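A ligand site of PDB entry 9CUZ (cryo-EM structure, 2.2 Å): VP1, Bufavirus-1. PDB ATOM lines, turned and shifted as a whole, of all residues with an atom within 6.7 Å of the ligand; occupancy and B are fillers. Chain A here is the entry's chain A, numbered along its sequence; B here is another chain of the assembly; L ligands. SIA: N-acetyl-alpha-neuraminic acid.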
ATOM      1  N   ARG A 506     -25.254   4.317 -11.497  1.00  0.00           N
ATOM      2  CA  ARG A 506     -25.880   5.611 -11.268  1.00  0.00           C
ATOM      3  C   ARG A 506     -27.270   5.549 -11.898  1.00  0.00           C
ATOM      4  O   ARG A 506     -27.403   5.436 -13.117  1.00  0.00           O
ATOM      5  CB  ARG A 506     -25.023   6.711 -11.879  1.00  0.00           C
ATOM      6  CG  ARG A 506     -23.661   6.774 -11.227  1.00  0.00           C
ATOM      7  CD  ARG A 506     -22.690   7.668 -11.961  1.00  0.00           C
ATOM      8  NE  ARG A 506     -22.949   9.095 -11.893  1.00  0.00           N
ATOM      9  CZ  ARG A 506     -22.482   9.874 -10.926  1.00  0.00           C
ATOM     10  NH1 ARG A 506     -22.734  11.173 -10.937  1.00  0.00           N
ATOM     11  NH2 ARG A 506     -21.756   9.359  -9.955  1.00  0.00           N
ATOM     12  N   LYS A 514     -27.794  17.648 -14.225  1.00  0.00           N
ATOM     13  CA  LYS A 514     -26.364  17.788 -14.006  1.00  0.00           C
ATOM     14  C   LYS A 514     -25.921  19.189 -14.392  1.00  0.00           C
ATOM     15  O   LYS A 514     -26.195  19.645 -15.507  1.00  0.00           O
ATOM     16  CB  LYS A 514     -25.582  16.737 -14.787  1.00  0.00           C
ATOM     17  CG  LYS A 514     -24.139  16.621 -14.388  1.00  0.00           C
ATOM     18  CD  LYS A 514     -23.475  15.516 -15.174  1.00  0.00           C
ATOM     19  CE  LYS A 514     -22.023  15.343 -14.842  1.00  0.00           C
ATOM     20  NZ  LYS A 514     -21.845  14.869 -13.455  1.00  0.00           N
ATOM     21  N   PHE A 517     -19.996  23.409 -14.909  1.00  0.00           N
ATOM     22  CA  PHE A 517     -19.687  24.793 -14.563  1.00  0.00           C
ATOM     23  C   PHE A 517     -18.186  25.022 -14.568  1.00  0.00           C
ATOM     24  O   PHE A 517     -17.388  24.097 -14.698  1.00  0.00           O
ATOM     25  CB  PHE A 517     -20.314  25.149 -13.219  1.00  0.00           C
ATOM     26  CG  PHE A 517     -19.957  24.198 -12.108  1.00  0.00           C
ATOM     27  CD1 PHE A 517     -18.853  24.413 -11.302  1.00  0.00           C
ATOM     28  CD2 PHE A 517     -20.717  23.064 -11.885  1.00  0.00           C
ATOM     29  CE1 PHE A 517     -18.521  23.524 -10.288  1.00  0.00           C
ATOM     30  CE2 PHE A 517     -20.397  22.170 -10.886  1.00  0.00           C
ATOM     31  CZ  PHE A 517     -19.299  22.394 -10.092  1.00  0.00           C
ATOM     32  N   GLY A 522     -18.098  28.726  -9.981  1.00  0.00           N
ATOM     33  CA  GLY A 522     -17.885  27.942  -8.775  1.00  0.00           C
ATOM     34  C   GLY A 522     -17.058  26.695  -8.916  1.00  0.00           C
ATOM     35  O   GLY A 522     -17.093  25.847  -8.021  1.00  0.00           O
ATOM     36  N   ASP A 523     -16.339  26.516 -10.011  1.00  0.00           N
ATOM     37  CA  ASP A 523     -15.292  25.518 -10.089  1.00  0.00           C
ATOM     38  C   ASP A 523     -13.999  26.106  -9.549  1.00  0.00           C
ATOM     39  O   ASP A 523     -13.748  27.306  -9.690  1.00  0.00           O
ATOM     40  CB  ASP A 523     -15.075  25.021 -11.516  1.00  0.00           C
ATOM     41  CG  ASP A 523     -14.112  23.851 -11.569  1.00  0.00           C
ATOM     42  OD1 ASP A 523     -13.695  23.366 -10.506  1.00  0.00           O
ATOM     43  OD2 ASP A 523     -13.750  23.430 -12.673  1.00  0.00           O
ATOM     44  N   ASP A 530     -15.983  21.918 -13.875  1.00  0.00           N
ATOM     45  CA  ASP A 530     -16.410  20.926 -12.849  1.00  0.00           C
ATOM     46  C   ASP A 530     -17.875  20.576 -13.123  1.00  0.00           C
ATOM     47  O   ASP A 530     -18.500  21.269 -13.960  1.00  0.00           O
ATOM     48  CB  ASP A 530     -16.199  21.461 -11.435  1.00  0.00           C
ATOM     49  CG  ASP A 530     -16.360  20.385 -10.366  1.00  0.00           C
ATOM     50  OD1 ASP A 530     -16.308  19.189 -10.727  1.00  0.00           O
ATOM     51  OD2 ASP A 530     -16.512  20.751  -9.184  1.00  0.00           O
ATOM     52  N   GLN A 531     -18.399  19.568 -12.441  1.00  0.00           N
ATOM     53  CA  GLN A 531     -19.786  19.126 -12.718  1.00  0.00           C
ATOM     54  C   GLN A 531     -20.410  18.554 -11.446  1.00  0.00           C
ATOM     55  O   GLN A 531     -19.702  17.849 -10.700  1.00  0.00           O
ATOM     56  CB  GLN A 531     -19.784  18.083 -13.835  1.00  0.00           C
ATOM     57  CG  GLN A 531     -18.983  16.831 -13.509  1.00  0.00           C
ATOM     58  CD  GLN A 531     -18.743  15.981 -14.730  1.00  0.00           C
ATOM     59  OE1 GLN A 531     -18.810  16.460 -15.861  1.00  0.00           O
ATOM     60  NE2 GLN A 531     -18.449  14.709 -14.508  1.00  0.00           N
ATOM     61  N   TRP A 532     -21.691  18.861 -11.203  1.00  0.00           N
ATOM     62  CA  TRP A 532     -22.399  18.287 -10.037  1.00  0.00           C
ATOM     63  C   TRP A 532     -23.653  17.569 -10.520  1.00  0.00           C
ATOM     64  O   TRP A 532     -24.503  18.230 -11.148  1.00  0.00           O
ATOM     65  CB  TRP A 532     -22.721  19.372  -8.998  1.00  0.00           C
ATOM     66  CG  TRP A 532     -23.515  18.851  -7.835  1.00  0.00           C
ATOM     67  CD1 TRP A 532     -24.863  18.837  -7.699  1.00  0.00           C
ATOM     68  CD2 TRP A 532     -22.976  18.255  -6.643  1.00  0.00           C
ATOM     69  NE1 TRP A 532     -25.212  18.282  -6.497  1.00  0.00           N
ATOM     70  CE2 TRP A 532     -24.078  17.906  -5.830  1.00  0.00           C
ATOM     71  CE3 TRP A 532     -21.690  17.972  -6.187  1.00  0.00           C
ATOM     72  CZ2 TRP A 532     -23.912  17.303  -4.586  1.00  0.00           C
ATOM     73  CZ3 TRP A 532     -21.525  17.370  -4.957  1.00  0.00           C
ATOM     74  CH2 TRP A 532     -22.633  17.034  -4.171  1.00  0.00           C
ATOM     75  N   TRP A 533     -23.763  16.260 -10.264  1.00  0.00           N
ATOM     76  CA  TRP A 533     -24.980  15.510 -10.632  1.00  0.00           C
ATOM     77  C   TRP A 533     -26.028  15.684  -9.535  1.00  0.00           C
ATOM     78  O   TRP A 533     -25.800  15.194  -8.410  1.00  0.00           O
ATOM     79  CB  TRP A 533     -24.670  14.031 -10.896  1.00  0.00           C
ATOM     80  CG  TRP A 533     -25.860  13.220 -11.303  1.00  0.00           C
ATOM     81  CD1 TRP A 533     -26.778  13.550 -12.249  1.00  0.00           C
ATOM     82  CD2 TRP A 533     -26.244  11.935 -10.793  1.00  0.00           C
ATOM     83  NE1 TRP A 533     -27.726  12.556 -12.356  1.00  0.00           N
ATOM     84  CE2 TRP A 533     -27.411  11.557 -11.474  1.00  0.00           C
ATOM     85  CE3 TRP A 533     -25.711  11.070  -9.830  1.00  0.00           C
ATOM     86  CZ2 TRP A 533     -28.068  10.352 -11.215  1.00  0.00           C
ATOM     87  CZ3 TRP A 533     -26.351   9.878  -9.577  1.00  0.00           C
ATOM     88  CH2 TRP A 533     -27.517   9.527 -10.268  1.00  0.00           C
ATOM     89  N   GLN A 534     -27.127  16.373  -9.836  1.00  0.00           N
ATOM     90  CA  GLN A 534     -28.200  16.620  -8.827  1.00  0.00           C
ATOM     91  C   GLN A 534     -29.225  15.486  -8.926  1.00  0.00           C
ATOM     92  O   GLN A 534     -30.067  15.542  -9.832  1.00  0.00           O
ATOM     93  CB  GLN A 534     -28.793  18.007  -9.050  1.00  0.00           C
ATOM     94  CG  GLN A 534     -29.254  18.684  -7.773  1.00  0.00           C
ATOM     95  CD  GLN A 534     -30.683  18.335  -7.445  1.00  0.00           C
ATOM     96  OE1 GLN A 534     -31.485  18.062  -8.342  1.00  0.00           O
ATOM     97  NE2 GLN A 534     -31.012  18.368  -6.169  1.00  0.00           N
ATOM     98  N   ASN A 535     -29.163  14.504  -8.005  1.00  0.00           N
ATOM     99  CA  ASN A 535     -30.034  13.292  -8.107  1.00  0.00           C
ATOM    100  C   ASN A 535     -31.268  13.411  -7.200  1.00  0.00           C
ATOM    101  O   ASN A 535     -32.127  12.512  -7.294  1.00  0.00           O
ATOM    102  CB  ASN A 535     -29.236  12.015  -7.850  1.00  0.00           C
ATOM    103  CG  ASN A 535     -28.404  12.071  -6.589  1.00  0.00           C
ATOM    104  OD1 ASN A 535     -28.517  13.000  -5.796  1.00  0.00           O
ATOM    105  ND2 ASN A 535     -27.557  11.071  -6.396  1.00  0.00           N
ATOM    106  N   TRP A 589     -26.113  26.820  -9.028  1.00  0.00           N
ATOM    107  CA  TRP A 589     -26.172  26.969 -10.471  1.00  0.00           C
ATOM    108  C   TRP A 589     -27.583  27.167 -10.994  1.00  0.00           C
ATOM    109  O   TRP A 589     -27.746  27.478 -12.172  1.00  0.00           O
ATOM    110  CB  TRP A 589     -25.535  25.748 -11.126  1.00  0.00           C
ATOM    111  CG  TRP A 589     -24.192  25.544 -10.559  1.00  0.00           C
ATOM    112  CD1 TRP A 589     -23.062  26.223 -10.860  1.00  0.00           C
ATOM    113  CD2 TRP A 589     -23.829  24.552  -9.598  1.00  0.00           C
ATOM    114  NE1 TRP A 589     -22.019  25.747 -10.121  1.00  0.00           N
ATOM    115  CE2 TRP A 589     -22.466  24.713  -9.345  1.00  0.00           C
ATOM    116  CE3 TRP A 589     -24.533  23.547  -8.933  1.00  0.00           C
ATOM    117  CZ2 TRP A 589     -21.777  23.917  -8.441  1.00  0.00           C
ATOM    118  CZ3 TRP A 589     -23.856  22.745  -8.043  1.00  0.00           C
ATOM    119  CH2 TRP A 589     -22.487  22.924  -7.801  1.00  0.00           C
ATOM    120  N   THR A 679     -18.433  15.451   0.893  1.00  0.00           N
ATOM    121  CA  THR A 679     -17.540  16.580   0.658  1.00  0.00           C
ATOM    122  C   THR A 679     -16.952  17.059   1.974  1.00  0.00           C
ATOM    123  O   THR A 679     -17.568  16.973   3.031  1.00  0.00           O
ATOM    124  CB  THR A 679     -18.273  17.737  -0.036  1.00  0.00           C
ATOM    125  OG1 THR A 679     -19.359  18.193   0.786  1.00  0.00           O
ATOM    126  CG2 THR A 679     -18.826  17.296  -1.368  1.00  0.00           C
ATOM    127  N   LYS A 683     -12.661  21.902   0.393  1.00  0.00           N
ATOM    128  CA  LYS A 683     -13.061  22.036  -1.036  1.00  0.00           C
ATOM    129  C   LYS A 683     -13.787  23.370  -1.264  1.00  0.00           C
ATOM    130  O   LYS A 683     -13.685  23.913  -2.383  1.00  0.00           O
ATOM    131  CB  LYS A 683     -13.973  20.869  -1.402  1.00  0.00           C
ATOM    132  CG  LYS A 683     -14.521  20.840  -2.825  1.00  0.00           C
ATOM    133  CD  LYS A 683     -15.655  19.838  -2.978  1.00  0.00           C
ATOM    134  CE  LYS A 683     -15.681  19.160  -4.328  1.00  0.00           C
ATOM    135  NZ  LYS A 683     -16.904  18.344  -4.491  1.00  0.00           N
ATOM    136  N   PHE A 684     -14.491  23.867  -0.246  1.00  0.00           N
ATOM    137  CA  PHE A 684     -15.299  25.099  -0.424  1.00  0.00           C
ATOM    138  C   PHE A 684     -14.579  26.292   0.223  1.00  0.00           C
ATOM    139  O   PHE A 684     -15.239  27.312   0.487  1.00  0.00           O
ATOM    140  CB  PHE A 684     -16.714  24.842   0.126  1.00  0.00           C
ATOM    141  CG  PHE A 684     -17.338  23.584  -0.413  1.00  0.00           C
ATOM    142  CD1 PHE A 684     -17.688  23.477  -1.740  1.00  0.00           C
ATOM    143  CD2 PHE A 684     -17.554  22.491   0.411  1.00  0.00           C
ATOM    144  CE1 PHE A 684     -18.264  22.318  -2.235  1.00  0.00           C
ATOM    145  CE2 PHE A 684     -18.135  21.327  -0.078  1.00  0.00           C
ATOM    146  CZ  PHE A 684     -18.484  21.244  -1.400  1.00  0.00           C
ATOM    147  N   GLU A 693     -14.416  26.079  -4.582  1.00  0.00           N
ATOM    148  CA  GLU A 693     -15.695  25.733  -5.183  1.00  0.00           C
ATOM    149  C   GLU A 693     -16.855  26.191  -4.316  1.00  0.00           C
ATOM    150  O   GLU A 693     -16.733  26.347  -3.104  1.00  0.00           O
ATOM    151  CB  GLU A 693     -15.813  24.225  -5.411  1.00  0.00           C
ATOM    152  CG  GLU A 693     -14.868  23.688  -6.450  1.00  0.00           C
ATOM    153  CD  GLU A 693     -15.018  22.212  -6.636  1.00  0.00           C
ATOM    154  OE1 GLU A 693     -15.732  21.588  -5.822  1.00  0.00           O
ATOM    155  OE2 GLU A 693     -14.405  21.649  -7.570  1.00  0.00           O
ATOM    156  N   LEU A 694     -17.921  26.421  -4.930  1.00  0.00           N
ATOM    157  CA  LEU A 694     -19.123  26.632  -4.138  1.00  0.00           C
ATOM    158  C   LEU A 694     -19.900  25.322  -3.957  1.00  0.00           C
ATOM    159  O   LEU A 694     -19.985  24.529  -4.894  1.00  0.00           O
ATOM    160  CB  LEU A 694     -20.017  27.692  -4.771  1.00  0.00           C
ATOM    161  CG  LEU A 694     -19.712  29.146  -4.421  1.00  0.00           C
ATOM    162  CD1 LEU A 694     -18.357  29.563  -4.928  1.00  0.00           C
ATOM    163  CD2 LEU A 694     -20.775  30.066  -4.986  1.00  0.00           C
ATOM    164  N   PRO A 695     -20.434  25.049  -2.775  1.00  0.00           N
ATOM    165  CA  PRO A 695     -21.185  23.812  -2.561  1.00  0.00           C
ATOM    166  C   PRO A 695     -22.595  23.846  -3.118  1.00  0.00           C
ATOM    167  O   PRO A 695     -23.289  24.869  -3.068  1.00  0.00           O
ATOM    168  CB  PRO A 695     -21.227  23.702  -1.037  1.00  0.00           C
ATOM    169  CG  PRO A 695     -21.190  25.111  -0.572  1.00  0.00           C
ATOM    170  CD  PRO A 695     -20.398  25.896  -1.577  1.00  0.00           C
ATOM    171  N   PHE A 696     -23.043  22.701  -3.615  1.00  0.00           N
ATOM    172  CA  PHE A 696     -24.464  22.529  -3.897  1.00  0.00           C
ATOM    173  C   PHE A 696     -25.261  22.557  -2.601  1.00  0.00           C
ATOM    174  O   PHE A 696     -24.873  21.921  -1.620  1.00  0.00           O
ATOM    175  CB  PHE A 696     -24.739  21.231  -4.653  1.00  0.00           C
ATOM    176  CG  PHE A 696     -26.209  20.917  -4.735  1.00  0.00           C
ATOM    177  CD1 PHE A 696     -27.027  21.574  -5.629  1.00  0.00           C
ATOM    178  CD2 PHE A 696     -26.767  19.978  -3.890  1.00  0.00           C
ATOM    179  CE1 PHE A 696     -28.374  21.299  -5.665  1.00  0.00           C
ATOM    180  CE2 PHE A 696     -28.120  19.700  -3.933  1.00  0.00           C
ATOM    181  CZ  PHE A 696     -28.915  20.360  -4.821  1.00  0.00           C
ATOM    182  N   ASP B 454     -27.344  12.325 -15.909  1.00  0.00           N
ATOM    183  CA  ASP B 454     -25.924  12.511 -15.510  1.00  0.00           C
ATOM    184  C   ASP B 454     -25.098  12.766 -16.774  1.00  0.00           C
ATOM    185  O   ASP B 454     -23.997  12.202 -16.883  1.00  0.00           O
ATOM    186  CB  ASP B 454     -25.426  11.308 -14.702  1.00  0.00           C
ATOM    187  CG  ASP B 454     -24.050  11.523 -14.089  1.00  0.00           C
ATOM    188  OD1 ASP B 454     -23.772  12.648 -13.648  1.00  0.00           O
ATOM    189  OD2 ASP B 454     -23.272  10.546 -14.077  1.00  0.00           O
ATOM    190  N   SER B 456     -22.799  15.006 -19.118  1.00  0.00           N
ATOM    191  CA  SER B 456     -21.923  16.184 -19.345  1.00  0.00           C
ATOM    192  C   SER B 456     -20.996  16.142 -20.553  1.00  0.00           C
ATOM    193  O   SER B 456     -20.728  17.214 -21.131  1.00  0.00           O
ATOM    194  CB  SER B 456     -21.130  16.246 -18.067  1.00  0.00           C
ATOM    195  OG  SER B 456     -20.208  15.161 -17.997  1.00  0.00           O
HETATM  196  C1  SIA L   1     -19.338  13.544 -11.176  1.00  0.00           C
HETATM  197  C2  SIA L   1     -18.292  14.051 -10.176  1.00  0.00           C
HETATM  198  C3  SIA L   1     -17.735  15.396 -10.567  1.00  0.00           C
HETATM  199  C4  SIA L   1     -17.231  16.168  -9.359  1.00  0.00           C
HETATM  200  C5  SIA L   1     -18.358  16.341  -8.346  1.00  0.00           C
HETATM  201  C6  SIA L   1     -19.495  15.377  -8.658  1.00  0.00           C
HETATM  202  C7  SIA L   1     -20.449  15.234  -7.479  1.00  0.00           C
HETATM  203  C8  SIA L   1     -21.667  14.367  -7.815  1.00  0.00           C
HETATM  204  C9  SIA L   1     -22.859  14.629  -6.929  1.00  0.00           C
HETATM  205  C10 SIA L   1     -18.217  18.710  -7.720  1.00  0.00           C
HETATM  206  C11 SIA L   1     -18.990  19.991  -7.568  1.00  0.00           C
HETATM  207  N5  SIA L   1     -18.850  17.715  -8.323  1.00  0.00           N
HETATM  208  O1A SIA L   1     -19.957  12.538 -10.928  1.00  0.00           O
HETATM  209  O1B SIA L   1     -19.543  14.152 -12.189  1.00  0.00           O
HETATM  210  O2  SIA L   1     -17.256  13.125 -10.084  1.00  0.00           O
HETATM  211  O4  SIA L   1     -16.152  15.459  -8.752  1.00  0.00           O
HETATM  212  O6  SIA L   1     -18.915  14.089  -8.891  1.00  0.00           O
HETATM  213  O7  SIA L   1     -19.761  14.679  -6.356  1.00  0.00           O
HETATM  214  O8  SIA L   1     -22.029  14.588  -9.174  1.00  0.00           O
HETATM  215  O9  SIA L   1     -23.960  13.792  -7.264  1.00  0.00           O
HETATM  216  O10 SIA L   1     -17.068  18.597  -7.298  1.00  0.00           O
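The backbone carbonyl oxygen (O) of Gln 531 lies within hydrogen-bond range of a nitrogen (N5) of the ligand, 2.5 Å away.
NE2 of Gln 531 is in hydrogen-bond range of O1B of the ligand, at 2.6 Å.
The backbone NH (N) of Trp 533 sits at hydrogen-bond distance from an oxygen (O8) of the ligand, at 2.6 Å.
The backbone carbonyl oxygen (O) of Trp 533 sits at hydrogen-bond distance from an oxygen (O9) of the ligand (2.6 Å).
NZ of Lys 514 is in salt-bridge range of O1B of the ligand (2.7 Å).
O10 of the ligand is in hydrogen-bond range of NZ of Lys 683 (2.8 Å).
NH1 of Arg 506 is in salt-bridge range of O1A of the ligand (3.1 Å).
The side-chain amide oxygen (OE1) of Gln 531 sits at hydrogen-bond distance from the side-chain hydroxyl (OG) of Ser 456 of chain B (2.9 Å).
The side-chain amino group (NZ) of Lys 514 lies within salt-bridge range of the side-chain carboxylate (OD1) of Asp 454 of chain B.
The side-chain amino group of Lys 683 lies within salt-bridge range of the side-chain carboxylate of Glu 693.
The backbone carbonyl oxygen of Phe 517 sits at hydrogen-bond distance from the backbone NH of Asp 530, at 2.7 Å.
The backbone NH of Asp 530 is in hydrogen-bond range of the side-chain carboxylate of Asp 523 (3.0 Å).
The guanidinium group of Arg 506 is in salt-bridge range of the side-chain carboxylate of Asp 454 of chain B, at 2.6 Å.
The side-chain carboxylate (OD2) of Asp 530 sits close to an oxygen (O10) of the ligand (2.9 Å).
Merely in contact with the ligand: Trp 532 (3.3 Å), Phe 517 (3.5 Å) and Glu 693 (3.6 Å).
Within 4 Å of the ligand: Arg 506, Lys 514, Phe 517, Asp 530, Gln 531, Trp 532, Trp 533, Lys 683 and Glu 693.
Along chain A the residues within 4 Å of the ligand span positions 506 to 693.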
